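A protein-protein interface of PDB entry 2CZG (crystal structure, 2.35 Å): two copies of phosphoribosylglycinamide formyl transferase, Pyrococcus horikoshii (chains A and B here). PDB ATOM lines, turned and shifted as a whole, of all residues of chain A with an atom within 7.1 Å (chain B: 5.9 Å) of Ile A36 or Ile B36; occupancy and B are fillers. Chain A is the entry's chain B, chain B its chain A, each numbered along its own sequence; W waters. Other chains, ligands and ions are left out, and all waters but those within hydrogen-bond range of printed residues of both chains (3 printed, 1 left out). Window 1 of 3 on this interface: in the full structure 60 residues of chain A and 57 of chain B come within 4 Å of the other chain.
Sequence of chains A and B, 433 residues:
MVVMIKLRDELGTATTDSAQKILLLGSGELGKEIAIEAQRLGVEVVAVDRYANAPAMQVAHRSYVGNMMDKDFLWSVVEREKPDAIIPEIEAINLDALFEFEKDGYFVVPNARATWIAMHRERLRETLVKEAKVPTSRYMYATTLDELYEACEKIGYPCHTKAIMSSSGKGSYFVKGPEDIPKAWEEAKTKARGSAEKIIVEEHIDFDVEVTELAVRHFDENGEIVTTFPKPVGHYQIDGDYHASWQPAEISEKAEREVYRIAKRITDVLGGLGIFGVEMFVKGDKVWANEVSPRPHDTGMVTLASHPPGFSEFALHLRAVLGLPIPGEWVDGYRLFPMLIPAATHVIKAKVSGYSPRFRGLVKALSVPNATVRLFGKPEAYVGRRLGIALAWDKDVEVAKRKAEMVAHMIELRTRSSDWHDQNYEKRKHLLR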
ATOM      1  N   LEU A  24       9.004  -9.259 -21.532  1.00  0.00           N
ATOM      2  CA  LEU A  24       9.153 -10.057 -20.327  1.00  0.00           C
ATOM      3  C   LEU A  24       8.652  -9.278 -19.119  1.00  0.00           C
ATOM      4  O   LEU A  24       9.171  -8.205 -18.804  1.00  0.00           O
ATOM      5  CB  LEU A  24      10.628 -10.416 -20.119  1.00  0.00           C
ATOM      6  CG  LEU A  24      11.316 -11.320 -21.155  1.00  0.00           C
ATOM      7  CD1 LEU A  24      12.832 -11.362 -20.901  1.00  0.00           C
ATOM      8  CD2 LEU A  24      10.754 -12.713 -21.048  1.00  0.00           C
ATOM      9  N   LEU A  30      15.263 -16.337 -14.650  1.00  0.00           N
ATOM     10  CA  LEU A  30      14.504 -17.102 -15.650  1.00  0.00           C
ATOM     11  C   LEU A  30      14.284 -16.264 -16.910  1.00  0.00           C
ATOM     12  O   LEU A  30      14.506 -16.725 -18.037  1.00  0.00           O
ATOM     13  CB  LEU A  30      13.159 -17.554 -15.056  1.00  0.00           C
ATOM     14  CG  LEU A  30      13.247 -18.349 -13.733  1.00  0.00           C
ATOM     15  CD1 LEU A  30      11.883 -18.952 -13.404  1.00  0.00           C
ATOM     16  CD2 LEU A  30      14.301 -19.466 -13.836  1.00  0.00           C
ATOM     17  N   GLY A  31      13.862 -15.021 -16.726  1.00  0.00           N
ATOM     18  CA  GLY A  31      13.672 -14.152 -17.871  1.00  0.00           C
ATOM     19  C   GLY A  31      15.004 -13.942 -18.579  1.00  0.00           C
ATOM     20  O   GLY A  31      15.066 -13.775 -19.803  1.00  0.00           O
ATOM     21  N   LYS A  32      16.086 -13.977 -17.811  1.00  0.00           N
ATOM     22  CA  LYS A  32      17.422 -13.761 -18.364  1.00  0.00           C
ATOM     23  C   LYS A  32      17.779 -14.776 -19.446  1.00  0.00           C
ATOM     24  O   LYS A  32      18.254 -14.404 -20.516  1.00  0.00           O
ATOM     25  CB  LYS A  32      18.481 -13.785 -17.245  1.00  0.00           C
ATOM     26  CG  LYS A  32      19.854 -13.248 -17.685  1.00  0.00           C
ATOM     27  CD  LYS A  32      20.892 -13.294 -16.559  1.00  0.00           C
ATOM     28  CE  LYS A  32      22.244 -12.720 -16.995  1.00  0.00           C
ATOM     29  NZ  LYS A  32      23.171 -12.570 -15.822  1.00  0.00           N
ATOM     30  N   GLU A  33      17.542 -16.052 -19.167  1.00  0.00           N
ATOM     31  CA  GLU A  33      17.847 -17.111 -20.129  1.00  0.00           C
ATOM     32  C   GLU A  33      16.876 -17.079 -21.302  1.00  0.00           C
ATOM     33  O   GLU A  33      17.240 -17.486 -22.404  1.00  0.00           O
ATOM     34  CB  GLU A  33      17.855 -18.489 -19.445  1.00  0.00           C
ATOM     35  CG  GLU A  33      19.126 -18.747 -18.650  1.00  0.00           C
ATOM     36  CD  GLU A  33      20.374 -18.868 -19.534  1.00  0.00           C
ATOM     37  OE1 GLU A  33      21.485 -18.760 -18.994  1.00  0.00           O
ATOM     38  OE2 GLU A  33      20.256 -19.082 -20.762  1.00  0.00           O
ATOM     39  N   ILE A  34      15.649 -16.598 -21.073  1.00  0.00           N
ATOM     40  CA  ILE A  34      14.666 -16.453 -22.162  1.00  0.00           C
ATOM     41  C   ILE A  34      15.259 -15.405 -23.097  1.00  0.00           C
ATOM     42  O   ILE A  34      15.291 -15.595 -24.319  1.00  0.00           O
ATOM     43  CB  ILE A  34      13.287 -15.924 -21.668  1.00  0.00           C
ATOM     44  CG1 ILE A  34      12.584 -17.002 -20.826  1.00  0.00           C
ATOM     45  CG2 ILE A  34      12.390 -15.591 -22.852  1.00  0.00           C
ATOM     46  CD1 ILE A  34      11.231 -16.585 -20.308  1.00  0.00           C
ATOM     47  N   ALA A  35      15.741 -14.311 -22.492  1.00  0.00           N
ATOM     48  CA  ALA A  35      16.362 -13.192 -23.212  1.00  0.00           C
ATOM     49  C   ALA A  35      17.573 -13.635 -24.015  1.00  0.00           C
ATOM     50  O   ALA A  35      17.781 -13.142 -25.120  1.00  0.00           O
ATOM     51  CB  ALA A  35      16.782 -12.079 -22.221  1.00  0.00           C
ATOM     52  N   ILE A  36      18.368 -14.561 -23.468  1.00  0.00           N
ATOM     53  CA  ILE A  36      19.558 -15.046 -24.171  1.00  0.00           C
ATOM     54  C   ILE A  36      19.197 -15.862 -25.429  1.00  0.00           C
ATOM     55  O   ILE A  36      19.796 -15.679 -26.491  1.00  0.00           O
ATOM     56  CB  ILE A  36      20.481 -15.864 -23.209  1.00  0.00           C
ATOM     57  CG1 ILE A  36      21.034 -14.898 -22.127  1.00  0.00           C
ATOM     58  CG2 ILE A  36      21.553 -16.621 -24.027  1.00  0.00           C
ATOM     59  CD1 ILE A  36      22.355 -15.263 -21.467  1.00  0.00           C
ATOM     60  N   GLU A  37      18.214 -16.753 -25.330  1.00  0.00           N
ATOM     61  CA  GLU A  37      17.827 -17.519 -26.502  1.00  0.00           C
ATOM     62  C   GLU A  37      17.162 -16.607 -27.527  1.00  0.00           C
ATOM     63  O   GLU A  37      17.318 -16.797 -28.727  1.00  0.00           O
ATOM     64  CB  GLU A  37      16.868 -18.651 -26.135  1.00  0.00           C
ATOM     65  CG  GLU A  37      16.476 -19.517 -27.346  1.00  0.00           C
ATOM     66  CD  GLU A  37      17.676 -20.214 -28.000  1.00  0.00           C
ATOM     67  OE1 GLU A  37      18.645 -20.585 -27.283  1.00  0.00           O
ATOM     68  OE2 GLU A  37      17.646 -20.409 -29.228  1.00  0.00           O
ATOM     69  N   ALA A  38      16.410 -15.617 -27.061  1.00  0.00           N
ATOM     70  CA  ALA A  38      15.768 -14.710 -27.995  1.00  0.00           C
ATOM     71  C   ALA A  38      16.856 -13.949 -28.788  1.00  0.00           C
ATOM     72  O   ALA A  38      16.753 -13.793 -30.011  1.00  0.00           O
ATOM     73  CB  ALA A  38      14.850 -13.740 -27.226  1.00  0.00           C
ATOM     74  N   GLN A  39      17.899 -13.493 -28.094  1.00  0.00           N
ATOM     75  CA  GLN A  39      19.013 -12.775 -28.736  1.00  0.00           C
ATOM     76  C   GLN A  39      19.729 -13.682 -29.726  1.00  0.00           C
ATOM     77  O   GLN A  39      20.205 -13.243 -30.778  1.00  0.00           O
ATOM     78  CB  GLN A  39      20.016 -12.304 -27.669  1.00  0.00           C
ATOM     79  CG  GLN A  39      19.508 -11.150 -26.820  1.00  0.00           C
ATOM     80  CD  GLN A  39      19.722  -9.817 -27.517  1.00  0.00           C
ATOM     81  OE1 GLN A  39      19.835  -9.755 -28.740  1.00  0.00           O
ATOM     82  NE2 GLN A  39      19.768  -8.749 -26.745  1.00  0.00           N
ATOM     83  N   ARG A  40      19.825 -14.960 -29.382  1.00  0.00           N
ATOM     84  CA  ARG A  40      20.493 -15.907 -30.266  1.00  0.00           C
ATOM     85  C   ARG A  40      19.668 -16.235 -31.518  1.00  0.00           C
ATOM     86  O   ARG A  40      20.168 -16.877 -32.437  1.00  0.00           O
ATOM     87  CB  ARG A  40      20.829 -17.182 -29.495  1.00  0.00           C
ATOM     88  CG  ARG A  40      22.087 -17.075 -28.658  1.00  0.00           C
ATOM     89  CD  ARG A  40      22.228 -18.277 -27.720  1.00  0.00           C
ATOM     90  NE  ARG A  40      23.604 -18.449 -27.275  1.00  0.00           N
ATOM     91  CZ  ARG A  40      23.976 -19.344 -26.370  1.00  0.00           C
ATOM     92  NH1 ARG A  40      23.059 -20.125 -25.821  1.00  0.00           N
ATOM     93  NH2 ARG A  40      25.258 -19.482 -26.038  1.00  0.00           N
ATOM     94  N   LEU A  41      18.407 -15.792 -31.541  1.00  0.00           N
ATOM     95  CA  LEU A  41      17.506 -16.011 -32.678  1.00  0.00           C
ATOM     96  C   LEU A  41      17.214 -14.689 -33.375  1.00  0.00           C
ATOM     97  O   LEU A  41      16.390 -14.623 -34.292  1.00  0.00           O
ATOM     98  CB  LEU A  41      16.193 -16.654 -32.221  1.00  0.00           C
ATOM     99  CG  LEU A  41      16.333 -18.105 -31.724  1.00  0.00           C
ATOM    100  CD1 LEU A  41      14.990 -18.641 -31.276  1.00  0.00           C
ATOM    101  CD2 LEU A  41      16.895 -18.960 -32.832  1.00  0.00           C
ATOM    102  N   GLY A  42      17.894 -13.635 -32.933  1.00  0.00           N
ATOM    103  CA  GLY A  42      17.720 -12.334 -33.546  1.00  0.00           C
ATOM    104  C   GLY A  42      16.370 -11.716 -33.233  1.00  0.00           C
ATOM    105  O   GLY A  42      15.874 -10.906 -34.000  1.00  0.00           O
ATOM    106  N   VAL A  45      14.079  -8.070 -27.590  1.00  0.00           N
ATOM    107  CA  VAL A  45      13.642  -8.302 -26.227  1.00  0.00           C
ATOM    108  C   VAL A  45      13.444  -7.029 -25.411  1.00  0.00           C
ATOM    109  O   VAL A  45      14.324  -6.171 -25.366  1.00  0.00           O
ATOM    110  CB  VAL A  45      14.684  -9.161 -25.468  1.00  0.00           C
ATOM    111  CG1 VAL A  45      14.124  -9.605 -24.131  1.00  0.00           C
ATOM    112  CG2 VAL A  45      15.120 -10.341 -26.314  1.00  0.00           C
ATOM    113  N   ALA A  56      17.524  -9.823 -16.668  1.00  0.00           N
ATOM    114  CA  ALA A  56      17.082  -9.858 -18.063  1.00  0.00           C
ATOM    115  C   ALA A  56      17.245  -8.534 -18.791  1.00  0.00           C
ATOM    116  O   ALA A  56      17.419  -8.523 -20.024  1.00  0.00           O
ATOM    117  CB  ALA A  56      15.641 -10.333 -18.158  1.00  0.00           C
ATOM    118  N   VAL A  59      20.592  -8.026 -20.459  1.00  0.00           N
ATOM    119  CA  VAL A  59      20.702  -8.749 -21.721  1.00  0.00           C
ATOM    120  C   VAL A  59      19.749  -8.241 -22.791  1.00  0.00           C
ATOM    121  O   VAL A  59      20.026  -8.392 -23.974  1.00  0.00           O
ATOM    122  CB  VAL A  59      20.420 -10.252 -21.504  1.00  0.00           C
ATOM    123  CG1 VAL A  59      20.174 -10.947 -22.848  1.00  0.00           C
ATOM    124  CG2 VAL A  59      21.599 -10.885 -20.786  1.00  0.00           C
ATOM    125  N   ALA A  60      18.639  -7.633 -22.372  1.00  0.00           N
ATOM    126  CA  ALA A  60      17.615  -7.134 -23.294  1.00  0.00           C
ATOM    127  C   ALA A  60      18.038  -5.963 -24.172  1.00  0.00           C
ATOM    128  O   ALA A  60      19.038  -5.312 -23.917  1.00  0.00           O
ATOM    129  CB  ALA A  60      16.374  -6.733 -22.505  1.00  0.00           C
ATOM    130  N   LEU A 318      10.162 -20.049 -25.298  1.00  0.00           N
ATOM    131  CA  LEU A 318      10.335 -19.045 -26.343  1.00  0.00           C
ATOM    132  C   LEU A 318       9.846 -19.548 -27.698  1.00  0.00           C
ATOM    133  O   LEU A 318       9.025 -18.908 -28.362  1.00  0.00           O
ATOM    134  CB  LEU A 318      11.820 -18.685 -26.476  1.00  0.00           C
ATOM    135  CG  LEU A 318      12.258 -17.241 -26.760  1.00  0.00           C
ATOM    136  CD1 LEU A 318      13.400 -17.272 -27.751  1.00  0.00           C
ATOM    137  CD2 LEU A 318      11.118 -16.398 -27.285  1.00  0.00           C
ATOM    138  N   ARG A 374      26.575 -19.948 -12.943  1.00  0.00           N
ATOM    139  CA  ARG A 374      25.912 -18.867 -13.628  1.00  0.00           C
ATOM    140  C   ARG A 374      25.707 -17.858 -12.502  1.00  0.00           C
ATOM    141  O   ARG A 374      25.197 -18.205 -11.434  1.00  0.00           O
ATOM    142  CB  ARG A 374      24.580 -19.359 -14.209  1.00  0.00           C
ATOM    143  CG  ARG A 374      24.762 -20.426 -15.297  1.00  0.00           C
ATOM    144  CD  ARG A 374      25.220 -19.756 -16.549  1.00  0.00           C
ATOM    145  NE  ARG A 374      25.731 -20.625 -17.610  1.00  0.00           N
ATOM    146  CZ  ARG A 374      27.024 -20.771 -17.906  1.00  0.00           C
ATOM    147  NH1 ARG A 374      27.969 -20.138 -17.214  1.00  0.00           N
ATOM    148  NH2 ARG A 374      27.377 -21.476 -18.966  1.00  0.00           N
ATOM    149  N   GLY B  31      32.036 -12.131 -31.062  1.00  0.00           N
ATOM    150  CA  GLY B  31      31.989 -11.272 -29.890  1.00  0.00           C
ATOM    151  C   GLY B  31      30.659 -11.463 -29.164  1.00  0.00           C
ATOM    152  O   GLY B  31      30.580 -11.392 -27.937  1.00  0.00           O
ATOM    153  N   LYS B  32      29.609 -11.737 -29.927  1.00  0.00           N
ATOM    154  CA  LYS B  32      28.276 -11.923 -29.349  1.00  0.00           C
ATOM    155  C   LYS B  32      28.244 -13.086 -28.351  1.00  0.00           C
ATOM    156  O   LYS B  32      27.714 -12.962 -27.248  1.00  0.00           O
ATOM    157  CB  LYS B  32      27.264 -12.157 -30.472  1.00  0.00           C
ATOM    158  CG  LYS B  32      25.823 -12.220 -30.022  1.00  0.00           C
ATOM    159  CD  LYS B  32      24.899 -12.527 -31.212  1.00  0.00           C
ATOM    160  CE  LYS B  32      23.442 -12.453 -30.798  1.00  0.00           C
ATOM    161  NZ  LYS B  32      22.509 -12.594 -31.951  1.00  0.00           N
ATOM    162  N   GLU B  33      28.794 -14.222 -28.746  1.00  0.00           N
ATOM    163  CA  GLU B  33      28.820 -15.362 -27.842  1.00  0.00           C
ATOM    164  C   GLU B  33      29.718 -15.103 -26.642  1.00  0.00           C
ATOM    165  O   GLU B  33      29.473 -15.641 -25.569  1.00  0.00           O
ATOM    166  CB  GLU B  33      29.235 -16.615 -28.593  1.00  0.00           C
ATOM    167  CG  GLU B  33      28.069 -17.196 -29.406  1.00  0.00           C
ATOM    168  CD  GLU B  33      26.995 -17.798 -28.512  1.00  0.00           C
ATOM    169  OE1 GLU B  33      25.854 -17.922 -28.978  1.00  0.00           O
ATOM    170  OE2 GLU B  33      27.291 -18.161 -27.342  1.00  0.00           O
ATOM    171  N   ILE B  34      30.741 -14.264 -26.813  1.00  0.00           N
ATOM    172  CA  ILE B  34      31.618 -13.944 -25.698  1.00  0.00           C
ATOM    173  C   ILE B  34      30.804 -13.083 -24.728  1.00  0.00           C
ATOM    174  O   ILE B  34      30.802 -13.325 -23.522  1.00  0.00           O
ATOM    175  CB  ILE B  34      32.882 -13.152 -26.156  1.00  0.00           C
ATOM    176  CG1 ILE B  34      33.835 -14.070 -26.924  1.00  0.00           C
ATOM    177  CG2 ILE B  34      33.633 -12.606 -24.944  1.00  0.00           C
ATOM    178  CD1 ILE B  34      35.089 -13.362 -27.414  1.00  0.00           C
ATOM    179  N   ALA B  35      30.098 -12.082 -25.260  1.00  0.00           N
ATOM    180  CA  ALA B  35      29.281 -11.212 -24.417  1.00  0.00           C
ATOM    181  C   ALA B  35      28.209 -12.038 -23.672  1.00  0.00           C
ATOM    182  O   ALA B  35      27.887 -11.753 -22.525  1.00  0.00           O
ATOM    183  CB  ALA B  35      28.631 -10.101 -25.272  1.00  0.00           C
ATOM    184  N   ILE B  36      27.671 -13.072 -24.319  1.00  0.00           N
ATOM    185  CA  ILE B  36      26.666 -13.903 -23.672  1.00  0.00           C
ATOM    186  C   ILE B  36      27.273 -14.655 -22.460  1.00  0.00           C
ATOM    187  O   ILE B  36      26.688 -14.671 -21.382  1.00  0.00           O
ATOM    188  CB  ILE B  36      26.037 -14.900 -24.684  1.00  0.00           C
ATOM    189  CG1 ILE B  36      25.037 -14.162 -25.584  1.00  0.00           C
ATOM    190  CG2 ILE B  36      25.312 -16.030 -23.944  1.00  0.00           C
ATOM    191  CD1 ILE B  36      24.488 -15.011 -26.722  1.00  0.00           C
ATOM    192  N   GLU B  37      28.449 -15.260 -22.620  1.00  0.00           N
ATOM    193  CA  GLU B  37      29.081 -15.947 -21.491  1.00  0.00           C
ATOM    194  C   GLU B  37      29.415 -14.958 -20.379  1.00  0.00           C
ATOM    195  O   GLU B  37      29.263 -15.255 -19.200  1.00  0.00           O
ATOM    196  CB  GLU B  37      30.373 -16.646 -21.904  1.00  0.00           C
ATOM    197  CG  GLU B  37      30.346 -18.152 -21.725  1.00  0.00           C
ATOM    198  CD  GLU B  37      29.815 -18.618 -20.369  1.00  0.00           C
ATOM    199  OE1 GLU B  37      28.839 -19.384 -20.383  1.00  0.00           O
ATOM    200  OE2 GLU B  37      30.357 -18.251 -19.305  1.00  0.00           O
ATOM    201  N   ALA B  38      29.880 -13.778 -20.753  1.00  0.00           N
ATOM    202  CA  ALA B  38      30.197 -12.792 -19.742  1.00  0.00           C
ATOM    203  C   ALA B  38      28.924 -12.423 -18.959  1.00  0.00           C
ATOM    204  O   ALA B  38      28.967 -12.333 -17.730  1.00  0.00           O
ATOM    205  CB  ALA B  38      30.827 -11.565 -20.396  1.00  0.00           C
ATOM    206  N   GLN B  39      27.800 -12.223 -19.659  1.00  0.00           N
ATOM    207  CA  GLN B  39      26.515 -11.884 -19.005  1.00  0.00           C
ATOM    208  C   GLN B  39      26.109 -13.024 -18.063  1.00  0.00           C
ATOM    209  O   GLN B  39      25.649 -12.801 -16.931  1.00  0.00           O
ATOM    210  CB  GLN B  39      25.420 -11.651 -20.069  1.00  0.00           C
ATOM    211  CG  GLN B  39      25.567 -10.332 -20.875  1.00  0.00           C
ATOM    212  CD  GLN B  39      24.963  -9.121 -20.147  1.00  0.00           C
ATOM    213  OE1 GLN B  39      24.698  -9.170 -18.945  1.00  0.00           O
ATOM    214  NE2 GLN B  39      24.755  -8.031 -20.878  1.00  0.00           N
ATOM    215  N   ARG B  40      26.303 -14.257 -18.519  1.00  0.00           N
ATOM    216  CA  ARG B  40      25.974 -15.409 -17.683  1.00  0.00           C
ATOM    217  C   ARG B  40      26.851 -15.476 -16.423  1.00  0.00           C
ATOM    218  O   ARG B  40      26.564 -16.240 -15.503  1.00  0.00           O
ATOM    219  CB  ARG B  40      26.124 -16.701 -18.493  1.00  0.00           C
ATOM    220  CG  ARG B  40      24.910 -16.976 -19.349  1.00  0.00           C
ATOM    221  CD  ARG B  40      25.142 -18.067 -20.376  1.00  0.00           C
ATOM    222  NE  ARG B  40      23.865 -18.600 -20.827  1.00  0.00           N
ATOM    223  CZ  ARG B  40      23.732 -19.579 -21.714  1.00  0.00           C
ATOM    224  NH1 ARG B  40      24.805 -20.128 -22.241  1.00  0.00           N
ATOM    225  NH2 ARG B  40      22.528 -20.006 -22.072  1.00  0.00           N
ATOM    226  N   LEU B  41      27.911 -14.672 -16.385  1.00  0.00           N
ATOM    227  CA  LEU B  41      28.816 -14.631 -15.246  1.00  0.00           C
ATOM    228  C   LEU B  41      28.707 -13.294 -14.518  1.00  0.00           C
ATOM    229  O   LEU B  41      29.443 -13.015 -13.563  1.00  0.00           O
ATOM    230  CB  LEU B  41      30.258 -14.868 -15.708  1.00  0.00           C
ATOM    231  CG  LEU B  41      30.551 -16.267 -16.270  1.00  0.00           C
ATOM    232  CD1 LEU B  41      32.044 -16.427 -16.629  1.00  0.00           C
ATOM    233  CD2 LEU B  41      30.156 -17.282 -15.206  1.00  0.00           C
ATOM    234  N   VAL B  59      23.599  -7.498 -27.116  1.00  0.00           N
ATOM    235  CA  VAL B  59      23.726  -8.286 -25.880  1.00  0.00           C
ATOM    236  C   VAL B  59      24.526  -7.581 -24.768  1.00  0.00           C
ATOM    237  O   VAL B  59      24.343  -7.867 -23.590  1.00  0.00           O
ATOM    238  CB  VAL B  59      24.403  -9.680 -26.182  1.00  0.00           C
ATOM    239  CG1 VAL B  59      24.886 -10.344 -24.893  1.00  0.00           C
ATOM    240  CG2 VAL B  59      23.395 -10.599 -26.849  1.00  0.00           C
HETATM  241  O   HOH W   1      24.759 -10.036 -16.123  1.00  0.00           O
HETATM  242  O   HOH W   2      20.120 -10.229 -31.593  1.00  0.00           O
HETATM  243  O   HOH W   3      23.657 -21.358 -19.024  1.00  0.00           O
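O of Gln A39 lies within hydrogen-bond range of NZ of Lys B32, at 2.7 Å.
The side-chain carboxylate (OE2) of Glu B33 lies within salt-bridge range of the guanidinium group (NH2) of Arg A40 (2.8 Å).
The side-chain carboxylate (OE1) of Glu B37 is in salt-bridge range of the guanidinium group (NH2) of Arg A374.
The backbone carbonyl oxygen of Gln B39 lies within hydrogen-bond range of the side-chain amino group of Lys A32, 2.7 Å away.
The side-chain carboxylate (OE2) of Glu A33 is in salt-bridge range of the guanidinium group (NH2) of Arg B40.
The side-chain amide nitrogen of Gln B39 sits at hydrogen-bond distance from the backbone carbonyl oxygen of Val B59 (2.7 Å).
The side-chain amide nitrogen of Gln A39 sits at hydrogen-bond distance from the backbone carbonyl oxygen of Val A59 (2.8 Å).
Ile A36 touches Ile B36.
Arg B40 touches Ile A36 (NE to CD1, 3.7 Å).
Val B59 touches Gln A39 (CG2 to CD, 3.8 Å).
Arg A40 touches Ile B36 (NE to CD1, 3.6 Å).
Arg A40 touches Arg B40 (NH1 to NH2, 3.8 Å).
Gln B39 touches Val A59 (CD to CG2, 3.9 Å).
CA of Arg A374 touches O of Arg B40, 3.3 Å away.
Printed residues of chain B within 4 Å of Ile A36: Ile B36 (3.8 Å) and Arg B40 (3.7 Å).
Of the printed residues of chain B, Gln A39 touches Lys B32 (2.7 Å) and Val B59 (3.8 Å).
Printed residues of chain B within 4 Å of Arg A374: Glu B37 (2.9 Å) and Arg B40 (3.3 Å).
Ile B36 touches just these residues of chain A: Ile A36 and Arg A40.
The nearest residue of chain B that does not touch Ile A36 is Gln B39 (4.9 Å).
The nearest printed residue of chain A that does not touch Gln B39 is Ile A36 (4.9 Å).
Hydrophobic or aromatic side chains of chain B within 4 Å of the printed part of chain A: Ile B36 and Val B59.
Among the printed residues, Asp or Glu carboxylates within 4 Å of a Lys or Arg side-chain nitrogen of the other chain: Glu A33 with Arg B40 (2.8 Å), Arg A40 with Glu B33 (2.8 Å) and Arg A374 with Glu B37 (2.9 Å).
Glu A33 touches Arg B40, and with the chains exchanged Arg A40 touches Glu B33.
Ile B36 touches its own counterpart, Ile A36.
Ile A36 touches Arg B40, and with the chains exchanged Arg A40 touches Ile B36.
Arg A40 touches its own counterpart, Arg B40.
Positions printed for both chains: 31, 32, 33, 34, 35, 36, 37, 38, 39, 40, 41 and 59.
Of the 12 pairs that touch across the chains among the printed residues, 10 have their exchanged pair printed and touching as well.
Water W3 lies within hydrogen-bond range of the guanidinium group of Arg A374 (2.6 Å), the guanidinium group of Arg B40 (3.3 Å) and the side-chain carboxylate of Glu A33 (3.4 Å).
Water W2 lies within hydrogen-bond range of OE1 of Gln A39 (2.9 Å) and NZ of Lys B32 (3.4 Å).
Water W1 lies within hydrogen-bond range of the side-chain amide oxygen of Gln B39 (3.0 Å) and the side-chain amino group of Lys A32 (3.0 Å).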
